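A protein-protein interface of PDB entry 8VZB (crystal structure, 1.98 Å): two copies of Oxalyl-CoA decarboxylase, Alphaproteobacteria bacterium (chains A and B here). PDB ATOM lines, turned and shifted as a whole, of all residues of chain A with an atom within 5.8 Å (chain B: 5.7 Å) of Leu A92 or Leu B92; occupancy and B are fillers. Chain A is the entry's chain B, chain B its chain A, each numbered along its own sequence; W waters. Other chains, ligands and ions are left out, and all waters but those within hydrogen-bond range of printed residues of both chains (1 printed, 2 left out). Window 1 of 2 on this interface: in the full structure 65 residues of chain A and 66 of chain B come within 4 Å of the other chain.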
ATOM      1  N   SER A  64      -0.118 -38.105  24.881  1.00  0.00           N
ATOM      2  CA  SER A  64      -0.143 -37.015  25.848  1.00  0.00           C
ATOM      3  C   SER A  64      -1.086 -37.324  27.004  1.00  0.00           C
ATOM      4  O   SER A  64      -0.887 -36.823  28.115  1.00  0.00           O
ATOM      5  CB  SER A  64      -0.534 -35.706  25.160  1.00  0.00           C
ATOM      6  OG  SER A  64      -1.864 -35.762  24.672  1.00  0.00           O
ATOM      7  N   GLY A  87       2.913 -32.799  15.429  1.00  0.00           N
ATOM      8  CA  GLY A  87       3.159 -33.597  16.619  1.00  0.00           C
ATOM      9  C   GLY A  87       2.784 -32.852  17.884  1.00  0.00           C
ATOM     10  O   GLY A  87       2.085 -33.382  18.752  1.00  0.00           O
ATOM     11  N   VAL A  88       3.222 -31.593  17.987  1.00  0.00           N
ATOM     12  CA  VAL A  88       2.896 -30.768  19.146  1.00  0.00           C
ATOM     13  C   VAL A  88       1.411 -30.430  19.161  1.00  0.00           C
ATOM     14  O   VAL A  88       0.762 -30.482  20.214  1.00  0.00           O
ATOM     15  CB  VAL A  88       3.764 -29.495  19.155  1.00  0.00           C
ATOM     16  CG1 VAL A  88       3.377 -28.579  20.315  1.00  0.00           C
ATOM     17  CG2 VAL A  88       5.236 -29.851  19.224  1.00  0.00           C
ATOM     18  N   VAL A  89       0.845 -30.078  18.001  1.00  0.00           N
ATOM     19  CA  VAL A  89      -0.559 -29.673  17.966  1.00  0.00           C
ATOM     20  C   VAL A  89      -1.456 -30.820  18.414  1.00  0.00           C
ATOM     21  O   VAL A  89      -2.393 -30.623  19.198  1.00  0.00           O
ATOM     22  CB  VAL A  89      -0.948 -29.161  16.566  1.00  0.00           C
ATOM     23  CG1 VAL A  89      -2.382 -28.651  16.586  1.00  0.00           C
ATOM     24  CG2 VAL A  89      -0.007 -28.050  16.116  1.00  0.00           C
ATOM     25  N   HIS A  90      -1.171 -32.039  17.944  1.00  0.00           N
ATOM     26  CA  HIS A  90      -1.925 -33.207  18.396  1.00  0.00           C
ATOM     27  C   HIS A  90      -1.829 -33.381  19.908  1.00  0.00           C
ATOM     28  O   HIS A  90      -2.801 -33.784  20.555  1.00  0.00           O
ATOM     29  CB  HIS A  90      -1.421 -34.469  17.695  1.00  0.00           C
ATOM     30  CG  HIS A  90      -1.882 -34.604  16.277  1.00  0.00           C
ATOM     31  ND1 HIS A  90      -1.770 -35.781  15.568  1.00  0.00           N
ATOM     32  CD2 HIS A  90      -2.455 -33.712  15.436  1.00  0.00           C
ATOM     33  CE1 HIS A  90      -2.256 -35.609  14.351  1.00  0.00           C
ATOM     34  NE2 HIS A  90      -2.678 -34.362  14.245  1.00  0.00           N
ATOM     35  N   ALA A  91      -0.666 -33.083  20.488  1.00  0.00           N
ATOM     36  CA  ALA A  91      -0.446 -33.289  21.911  1.00  0.00           C
ATOM     37  C   ALA A  91      -1.036 -32.185  22.774  1.00  0.00           C
ATOM     38  O   ALA A  91      -1.034 -32.320  24.003  1.00  0.00           O
ATOM     39  CB  ALA A  91       1.051 -33.415  22.201  1.00  0.00           C
ATOM     40  N   LEU A  92      -1.529 -31.100  22.172  1.00  0.00           N
ATOM     41  CA  LEU A  92      -2.172 -30.049  22.954  1.00  0.00           C
ATOM     42  C   LEU A  92      -3.363 -30.574  23.738  1.00  0.00           C
ATOM     43  O   LEU A  92      -3.716 -29.994  24.771  1.00  0.00           O
ATOM     44  CB  LEU A  92      -2.620 -28.905  22.043  1.00  0.00           C
ATOM     45  CG  LEU A  92      -1.515 -28.203  21.251  1.00  0.00           C
ATOM     46  CD1 LEU A  92      -2.106 -27.111  20.369  1.00  0.00           C
ATOM     47  CD2 LEU A  92      -0.457 -27.635  22.186  1.00  0.00           C
ATOM     48  N   ALA A  93      -3.984 -31.659  23.273  1.00  0.00           N
ATOM     49  CA  ALA A  93      -5.107 -32.246  23.997  1.00  0.00           C
ATOM     50  C   ALA A  93      -4.701 -32.643  25.412  1.00  0.00           C
ATOM     51  O   ALA A  93      -5.418 -32.359  26.379  1.00  0.00           O
ATOM     52  CB  ALA A  93      -5.644 -33.456  23.232  1.00  0.00           C
ATOM     53  N   GLY A  94      -3.549 -33.304  25.550  1.00  0.00           N
ATOM     54  CA  GLY A  94      -3.111 -33.736  26.866  1.00  0.00           C
ATOM     55  C   GLY A  94      -2.719 -32.581  27.767  1.00  0.00           C
ATOM     56  O   GLY A  94      -2.964 -32.619  28.979  1.00  0.00           O
ATOM     57  N   LEU A  95      -2.090 -31.547  27.201  1.00  0.00           N
ATOM     58  CA  LEU A  95      -1.776 -30.362  27.995  1.00  0.00           C
ATOM     59  C   LEU A  95      -3.042 -29.765  28.591  1.00  0.00           C
ATOM     60  O   LEU A  95      -3.099 -29.465  29.790  1.00  0.00           O
ATOM     61  CB  LEU A  95      -1.048 -29.325  27.139  1.00  0.00           C
ATOM     62  CG  LEU A  95       0.277 -29.730  26.487  1.00  0.00           C
ATOM     63  CD1 LEU A  95       0.813 -28.581  25.649  1.00  0.00           C
ATOM     64  CD2 LEU A  95       1.298 -30.147  27.536  1.00  0.00           C
ATOM     65  N   ALA A  96      -4.079 -29.600  27.766  1.00  0.00           N
ATOM     66  CA  ALA A  96      -5.333 -29.031  28.249  1.00  0.00           C
ATOM     67  C   ALA A  96      -5.947 -29.896  29.342  1.00  0.00           C
ATOM     68  O   ALA A  96      -6.407 -29.381  30.365  1.00  0.00           O
ATOM     69  CB  ALA A  96      -6.312 -28.860  27.085  1.00  0.00           C
ATOM     70  N   ASN A  97      -5.960 -31.217  29.143  1.00  0.00           N
ATOM     71  CA  ASN A  97      -6.564 -32.103  30.132  1.00  0.00           C
ATOM     72  C   ASN A  97      -5.756 -32.122  31.425  1.00  0.00           C
ATOM     73  O   ASN A  97      -6.326 -32.198  32.519  1.00  0.00           O
ATOM     74  CB  ASN A  97      -6.701 -33.512  29.554  1.00  0.00           C
ATOM     75  CG  ASN A  97      -7.629 -34.388  30.369  1.00  0.00           C
ATOM     76  OD1 ASN A  97      -8.849 -34.251  30.297  1.00  0.00           O
ATOM     77  ND2 ASN A  97      -7.054 -35.300  31.148  1.00  0.00           N
ATOM     78  N   LEU A 107       5.721 -32.407  28.368  1.00  0.00           N
ATOM     79  CA  LEU A 107       5.689 -32.615  26.928  1.00  0.00           C
ATOM     80  C   LEU A 107       7.011 -32.136  26.340  1.00  0.00           C
ATOM     81  O   LEU A 107       7.387 -30.973  26.514  1.00  0.00           O
ATOM     82  CB  LEU A 107       4.511 -31.875  26.294  1.00  0.00           C
ATOM     83  CG  LEU A 107       4.437 -31.914  24.766  1.00  0.00           C
ATOM     84  CD1 LEU A 107       4.356 -33.344  24.275  1.00  0.00           C
ATOM     85  CD2 LEU A 107       3.250 -31.106  24.263  1.00  0.00           C
ATOM     86  N   LEU A 130       1.843 -21.710  21.018  1.00  0.00           N
ATOM     87  CA  LEU A 130       0.617 -22.502  21.007  1.00  0.00           C
ATOM     88  C   LEU A 130       0.405 -23.217  22.336  1.00  0.00           C
ATOM     89  O   LEU A 130      -0.728 -23.316  22.818  1.00  0.00           O
ATOM     90  CB  LEU A 130       0.652 -23.517  19.862  1.00  0.00           C
ATOM     91  CG  LEU A 130       0.694 -22.985  18.431  1.00  0.00           C
ATOM     92  CD1 LEU A 130       0.755 -24.134  17.437  1.00  0.00           C
ATOM     93  CD2 LEU A 130      -0.514 -22.100  18.153  1.00  0.00           C
ATOM     94  N   ALA A 131       1.484 -23.716  22.942  1.00  0.00           N
ATOM     95  CA  ALA A 131       1.366 -24.509  24.160  1.00  0.00           C
ATOM     96  C   ALA A 131       1.179 -23.652  25.405  1.00  0.00           C
ATOM     97  O   ALA A 131       0.569 -24.115  26.376  1.00  0.00           O
ATOM     98  CB  ALA A 131       2.604 -25.392  24.334  1.00  0.00           C
ATOM     99  N   LEU A 134      -1.863 -23.463  27.820  1.00  0.00           N
ATOM    100  CA  LEU A 134      -2.239 -24.722  28.449  1.00  0.00           C
ATOM    101  C   LEU A 134      -1.180 -25.248  29.408  1.00  0.00           C
ATOM    102  O   LEU A 134      -1.310 -26.375  29.897  1.00  0.00           O
ATOM    103  CB  LEU A 134      -2.534 -25.775  27.380  1.00  0.00           C
ATOM    104  CG  LEU A 134      -3.598 -25.427  26.339  1.00  0.00           C
ATOM    105  CD1 LEU A 134      -3.596 -26.465  25.229  1.00  0.00           C
ATOM    106  CD2 LEU A 134      -4.974 -25.324  26.981  1.00  0.00           C
ATOM    107  N   SER B  64     -11.664 -32.585  11.771  1.00  0.00           N
ATOM    108  CA  SER B  64     -11.119 -31.300  11.350  1.00  0.00           C
ATOM    109  C   SER B  64     -10.286 -31.440  10.084  1.00  0.00           C
ATOM    110  O   SER B  64     -10.227 -30.507   9.278  1.00  0.00           O
ATOM    111  CB  SER B  64     -10.292 -30.675  12.474  1.00  0.00           C
ATOM    112  OG  SER B  64      -9.131 -31.441  12.748  1.00  0.00           O
ATOM    113  N   GLY B  87     -13.225 -31.072  22.777  1.00  0.00           N
ATOM    114  CA  GLY B  87     -13.618 -31.147  21.379  1.00  0.00           C
ATOM    115  C   GLY B  87     -12.882 -30.130  20.528  1.00  0.00           C
ATOM    116  O   GLY B  87     -12.363 -30.453  19.454  1.00  0.00           O
ATOM    117  N   VAL B  88     -12.813 -28.886  21.008  1.00  0.00           N
ATOM    118  CA  VAL B  88     -12.088 -27.841  20.295  1.00  0.00           C
ATOM    119  C   VAL B  88     -10.590 -28.123  20.302  1.00  0.00           C
ATOM    120  O   VAL B  88      -9.916 -27.982  19.275  1.00  0.00           O
ATOM    121  CB  VAL B  88     -12.399 -26.461  20.906  1.00  0.00           C
ATOM    122  CG1 VAL B  88     -11.486 -25.397  20.308  1.00  0.00           C
ATOM    123  CG2 VAL B  88     -13.862 -26.097  20.697  1.00  0.00           C
ATOM    124  N   VAL B  89     -10.043 -28.513  21.457  1.00  0.00           N
ATOM    125  CA  VAL B  89      -8.602 -28.742  21.553  1.00  0.00           C
ATOM    126  C   VAL B  89      -8.182 -29.887  20.638  1.00  0.00           C
ATOM    127  O   VAL B  89      -7.127 -29.827  19.994  1.00  0.00           O
ATOM    128  CB  VAL B  89      -8.185 -29.000  23.013  1.00  0.00           C
ATOM    129  CG1 VAL B  89      -6.671 -29.149  23.106  1.00  0.00           C
ATOM    130  CG2 VAL B  89      -8.650 -27.866  23.914  1.00  0.00           C
ATOM    131  N   HIS B  90      -8.996 -30.946  20.562  1.00  0.00           N
ATOM    132  CA  HIS B  90      -8.734 -32.005  19.591  1.00  0.00           C
ATOM    133  C   HIS B  90      -8.777 -31.473  18.163  1.00  0.00           C
ATOM    134  O   HIS B  90      -8.044 -31.963  17.296  1.00  0.00           O
ATOM    135  CB  HIS B  90      -9.749 -33.141  19.744  1.00  0.00           C
ATOM    136  CG  HIS B  90      -9.526 -34.005  20.948  1.00  0.00           C
ATOM    137  ND1 HIS B  90     -10.114 -35.243  21.091  1.00  0.00           N
ATOM    138  CD2 HIS B  90      -8.791 -33.808  22.067  1.00  0.00           C
ATOM    139  CE1 HIS B  90      -9.747 -35.775  22.243  1.00  0.00           C
ATOM    140  NE2 HIS B  90      -8.942 -34.925  22.855  1.00  0.00           N
ATOM    141  N   ALA B  91      -9.624 -30.477  17.902  1.00  0.00           N
ATOM    142  CA  ALA B  91      -9.796 -29.949  16.554  1.00  0.00           C
ATOM    143  C   ALA B  91      -8.705 -28.970  16.148  1.00  0.00           C
ATOM    144  O   ALA B  91      -8.608 -28.639  14.961  1.00  0.00           O
ATOM    145  CB  ALA B  91     -11.163 -29.270  16.427  1.00  0.00           C
ATOM    146  N   LEU B  92      -7.887 -28.501  17.096  1.00  0.00           N
ATOM    147  CA  LEU B  92      -6.813 -27.573  16.750  1.00  0.00           C
ATOM    148  C   LEU B  92      -5.871 -28.174  15.717  1.00  0.00           C
ATOM    149  O   LEU B  92      -5.235 -27.439  14.951  1.00  0.00           O
ATOM    150  CB  LEU B  92      -6.036 -27.168  18.001  1.00  0.00           C
ATOM    151  CG  LEU B  92      -6.816 -26.392  19.063  1.00  0.00           C
ATOM    152  CD1 LEU B  92      -5.917 -26.036  20.244  1.00  0.00           C
ATOM    153  CD2 LEU B  92      -7.440 -25.139  18.467  1.00  0.00           C
ATOM    154  N   ALA B  93      -5.779 -29.506  15.677  1.00  0.00           N
ATOM    155  CA  ALA B  93      -4.966 -30.183  14.672  1.00  0.00           C
ATOM    156  C   ALA B  93      -5.314 -29.713  13.263  1.00  0.00           C
ATOM    157  O   ALA B  93      -4.429 -29.359  12.474  1.00  0.00           O
ATOM    158  CB  ALA B  93      -5.148 -31.698  14.794  1.00  0.00           C
ATOM    159  N   GLY B  94      -6.608 -29.681  12.939  1.00  0.00           N
ATOM    160  CA  GLY B  94      -7.015 -29.323  11.590  1.00  0.00           C
ATOM    161  C   GLY B  94      -6.844 -27.846  11.291  1.00  0.00           C
ATOM    162  O   GLY B  94      -6.525 -27.467  10.158  1.00  0.00           O
ATOM    163  N   LEU B  95      -7.061 -26.991  12.292  1.00  0.00           N
ATOM    164  CA  LEU B  95      -6.841 -25.561  12.099  1.00  0.00           C
ATOM    165  C   LEU B  95      -5.401 -25.283  11.685  1.00  0.00           C
ATOM    166  O   LEU B  95      -5.149 -24.537  10.734  1.00  0.00           O
ATOM    167  CB  LEU B  95      -7.184 -24.797  13.377  1.00  0.00           C
ATOM    168  CG  LEU B  95      -8.615 -24.868  13.905  1.00  0.00           C
ATOM    169  CD1 LEU B  95      -8.739 -24.015  15.156  1.00  0.00           C
ATOM    170  CD2 LEU B  95      -9.608 -24.421  12.845  1.00  0.00           C
ATOM    171  N   ALA B  96      -4.441 -25.885  12.392  1.00  0.00           N
ATOM    172  CA  ALA B  96      -3.035 -25.673  12.069  1.00  0.00           C
ATOM    173  C   ALA B  96      -2.709 -26.176  10.669  1.00  0.00           C
ATOM    174  O   ALA B  96      -2.026 -25.490   9.899  1.00  0.00           O
ATOM    175  CB  ALA B  96      -2.147 -26.363  13.107  1.00  0.00           C
ATOM    176  N   ASN B  97      -3.197 -27.371  10.321  1.00  0.00           N
ATOM    177  CA  ASN B  97      -2.940 -27.924   8.996  1.00  0.00           C
ATOM    178  C   ASN B  97      -3.561 -27.057   7.907  1.00  0.00           C
ATOM    179  O   ASN B  97      -2.953 -26.845   6.852  1.00  0.00           O
ATOM    180  CB  ASN B  97      -3.472 -29.355   8.907  1.00  0.00           C
ATOM    181  CG  ASN B  97      -2.824 -30.149   7.790  1.00  0.00           C
ATOM    182  OD1 ASN B  97      -1.673 -30.566   7.904  1.00  0.00           O
ATOM    183  ND2 ASN B  97      -3.560 -30.367   6.708  1.00  0.00           N
ATOM    184  N   LEU B 107     -14.534 -24.107  11.601  1.00  0.00           N
ATOM    185  CA  LEU B 107     -14.690 -24.899  12.813  1.00  0.00           C
ATOM    186  C   LEU B 107     -15.756 -24.252  13.687  1.00  0.00           C
ATOM    187  O   LEU B 107     -15.653 -23.066  14.030  1.00  0.00           O
ATOM    188  CB  LEU B 107     -13.364 -25.016  13.563  1.00  0.00           C
ATOM    189  CG  LEU B 107     -13.389 -25.711  14.929  1.00  0.00           C
ATOM    190  CD1 LEU B 107     -13.934 -27.130  14.836  1.00  0.00           C
ATOM    191  CD2 LEU B 107     -11.998 -25.711  15.548  1.00  0.00           C
ATOM    192  N   LEU B 130      -7.382 -20.045  22.421  1.00  0.00           N
ATOM    193  CA  LEU B 130      -6.560 -21.172  21.997  1.00  0.00           C
ATOM    194  C   LEU B 130      -6.495 -21.274  20.478  1.00  0.00           C
ATOM    195  O   LEU B 130      -5.449 -21.621  19.918  1.00  0.00           O
ATOM    196  CB  LEU B 130      -7.102 -22.471  22.593  1.00  0.00           C
ATOM    197  CG  LEU B 130      -7.055 -22.607  24.116  1.00  0.00           C
ATOM    198  CD1 LEU B 130      -7.707 -23.905  24.567  1.00  0.00           C
ATOM    199  CD2 LEU B 130      -5.619 -22.540  24.601  1.00  0.00           C
ATOM    200  N   ALA B 131      -7.599 -20.972  19.796  1.00  0.00           N
ATOM    201  CA  ALA B 131      -7.667 -21.180  18.354  1.00  0.00           C
ATOM    202  C   ALA B 131      -7.076 -20.015  17.571  1.00  0.00           C
ATOM    203  O   ALA B 131      -6.609 -20.210  16.443  1.00  0.00           O
ATOM    204  CB  ALA B 131      -9.116 -21.410  17.931  1.00  0.00           C
ATOM    205  N   LEU B 134      -4.060 -19.990  15.220  1.00  0.00           N
ATOM    206  CA  LEU B 134      -4.153 -20.931  14.115  1.00  0.00           C
ATOM    207  C   LEU B 134      -5.201 -20.534  13.082  1.00  0.00           C
ATOM    208  O   LEU B 134      -5.444 -21.298  12.142  1.00  0.00           O
ATOM    209  CB  LEU B 134      -4.455 -22.333  14.652  1.00  0.00           C
ATOM    210  CG  LEU B 134      -3.436 -22.897  15.641  1.00  0.00           C
ATOM    211  CD1 LEU B 134      -3.909 -24.222  16.228  1.00  0.00           C
ATOM    212  CD2 LEU B 134      -2.085 -23.062  14.966  1.00  0.00           C
HETATM  213  O   HOH W   1      -5.683 -33.850  18.612  1.00  0.00           O
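Val A89 touches Leu B92, and with the chains exchanged Leu A92 touches Val B89. Val A89 touches Ala B93, and with the chains exchanged Ala A93 touches Val B89. His A90 touches Ala B93, and with the chains exchanged Ala A93 touches His B90. Leu B92 touches its own counterpart, Leu A92. Positions printed for both chains: 64, 87, 88, 89, 90, 91, 92, 93, 94, 95, 96, 97, 107, 130, 131 and 134.
Printed residues of chain B within 4 Å of Val A89: Leu B92 (3.5 Å) and Ala B93 (3.6 Å). Printed residues of chain B within 4 Å of His A90: Ala B93. Of chain B, only Val B89 and Leu B92 come within 4 Å of Leu A92. Of the printed residues of chain B, Ala A93 touches Val B89 (3.6 Å) and His B90 (3.4 Å). Printed residues of chain A within 4 Å of Val B89: Leu A92 (3.5 Å) and Ala A93 (3.6 Å). Of chain A, only Val A89 (3.5 Å) and Leu A92 (3.96 Å) come within 4 Å of Leu B92. Leu B95 touches none of the printed residues of chain A. Asn B97 touches none of the printed residues of chain A. The nearest residue of chain B that does not touch Leu A92 is Leu B134 (5.4 Å). The nearest residue of chain A that does not touch Leu B92 is Leu A134 (5.5 Å). The nearest printed residue of chain B that does not touch His A90 is Val B89 (5.9 Å).
Water W1 lies within hydrogen-bond range of the backbone carbonyl oxygen (O) of His B90 (3.3 Å) and the backbone carbonyl oxygen (O) of His A90 (3.5 Å).
Among the printed residues, merely in contact across the chains: Val A89 with Leu B92, Val A89 with Ala B93, His A90 with Ala B93, Leu A92 with Val B89, Leu A92 with Leu B92, Ala A93 with Val B89, Ala A93 with His B90, Leu A130 with Leu B134 and Leu A134 with Leu B130.
Of the 16 printed residues of chain A, 6 touch a printed residue of chain B. Printed residues of chain A that touch a printed residue of chain B: Val A89, His A90, Leu A92, Ala A93, Leu A130 and Leu A134. Hydrophobic or aromatic side chains of chain A within 4 Å of the printed part of chain B: Val A89, His A90, Leu A92, Ala A93, Leu A130 and Leu A134. Of the 16 printed residues of chain B, 6 touch a printed residue of chain A. Among the printed residues, 9 pairs touch across the chains. Among the printed residues, no Asp or Glu carboxylate lies within 4 Å of a Lys or Arg side-chain nitrogen of the other chain.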
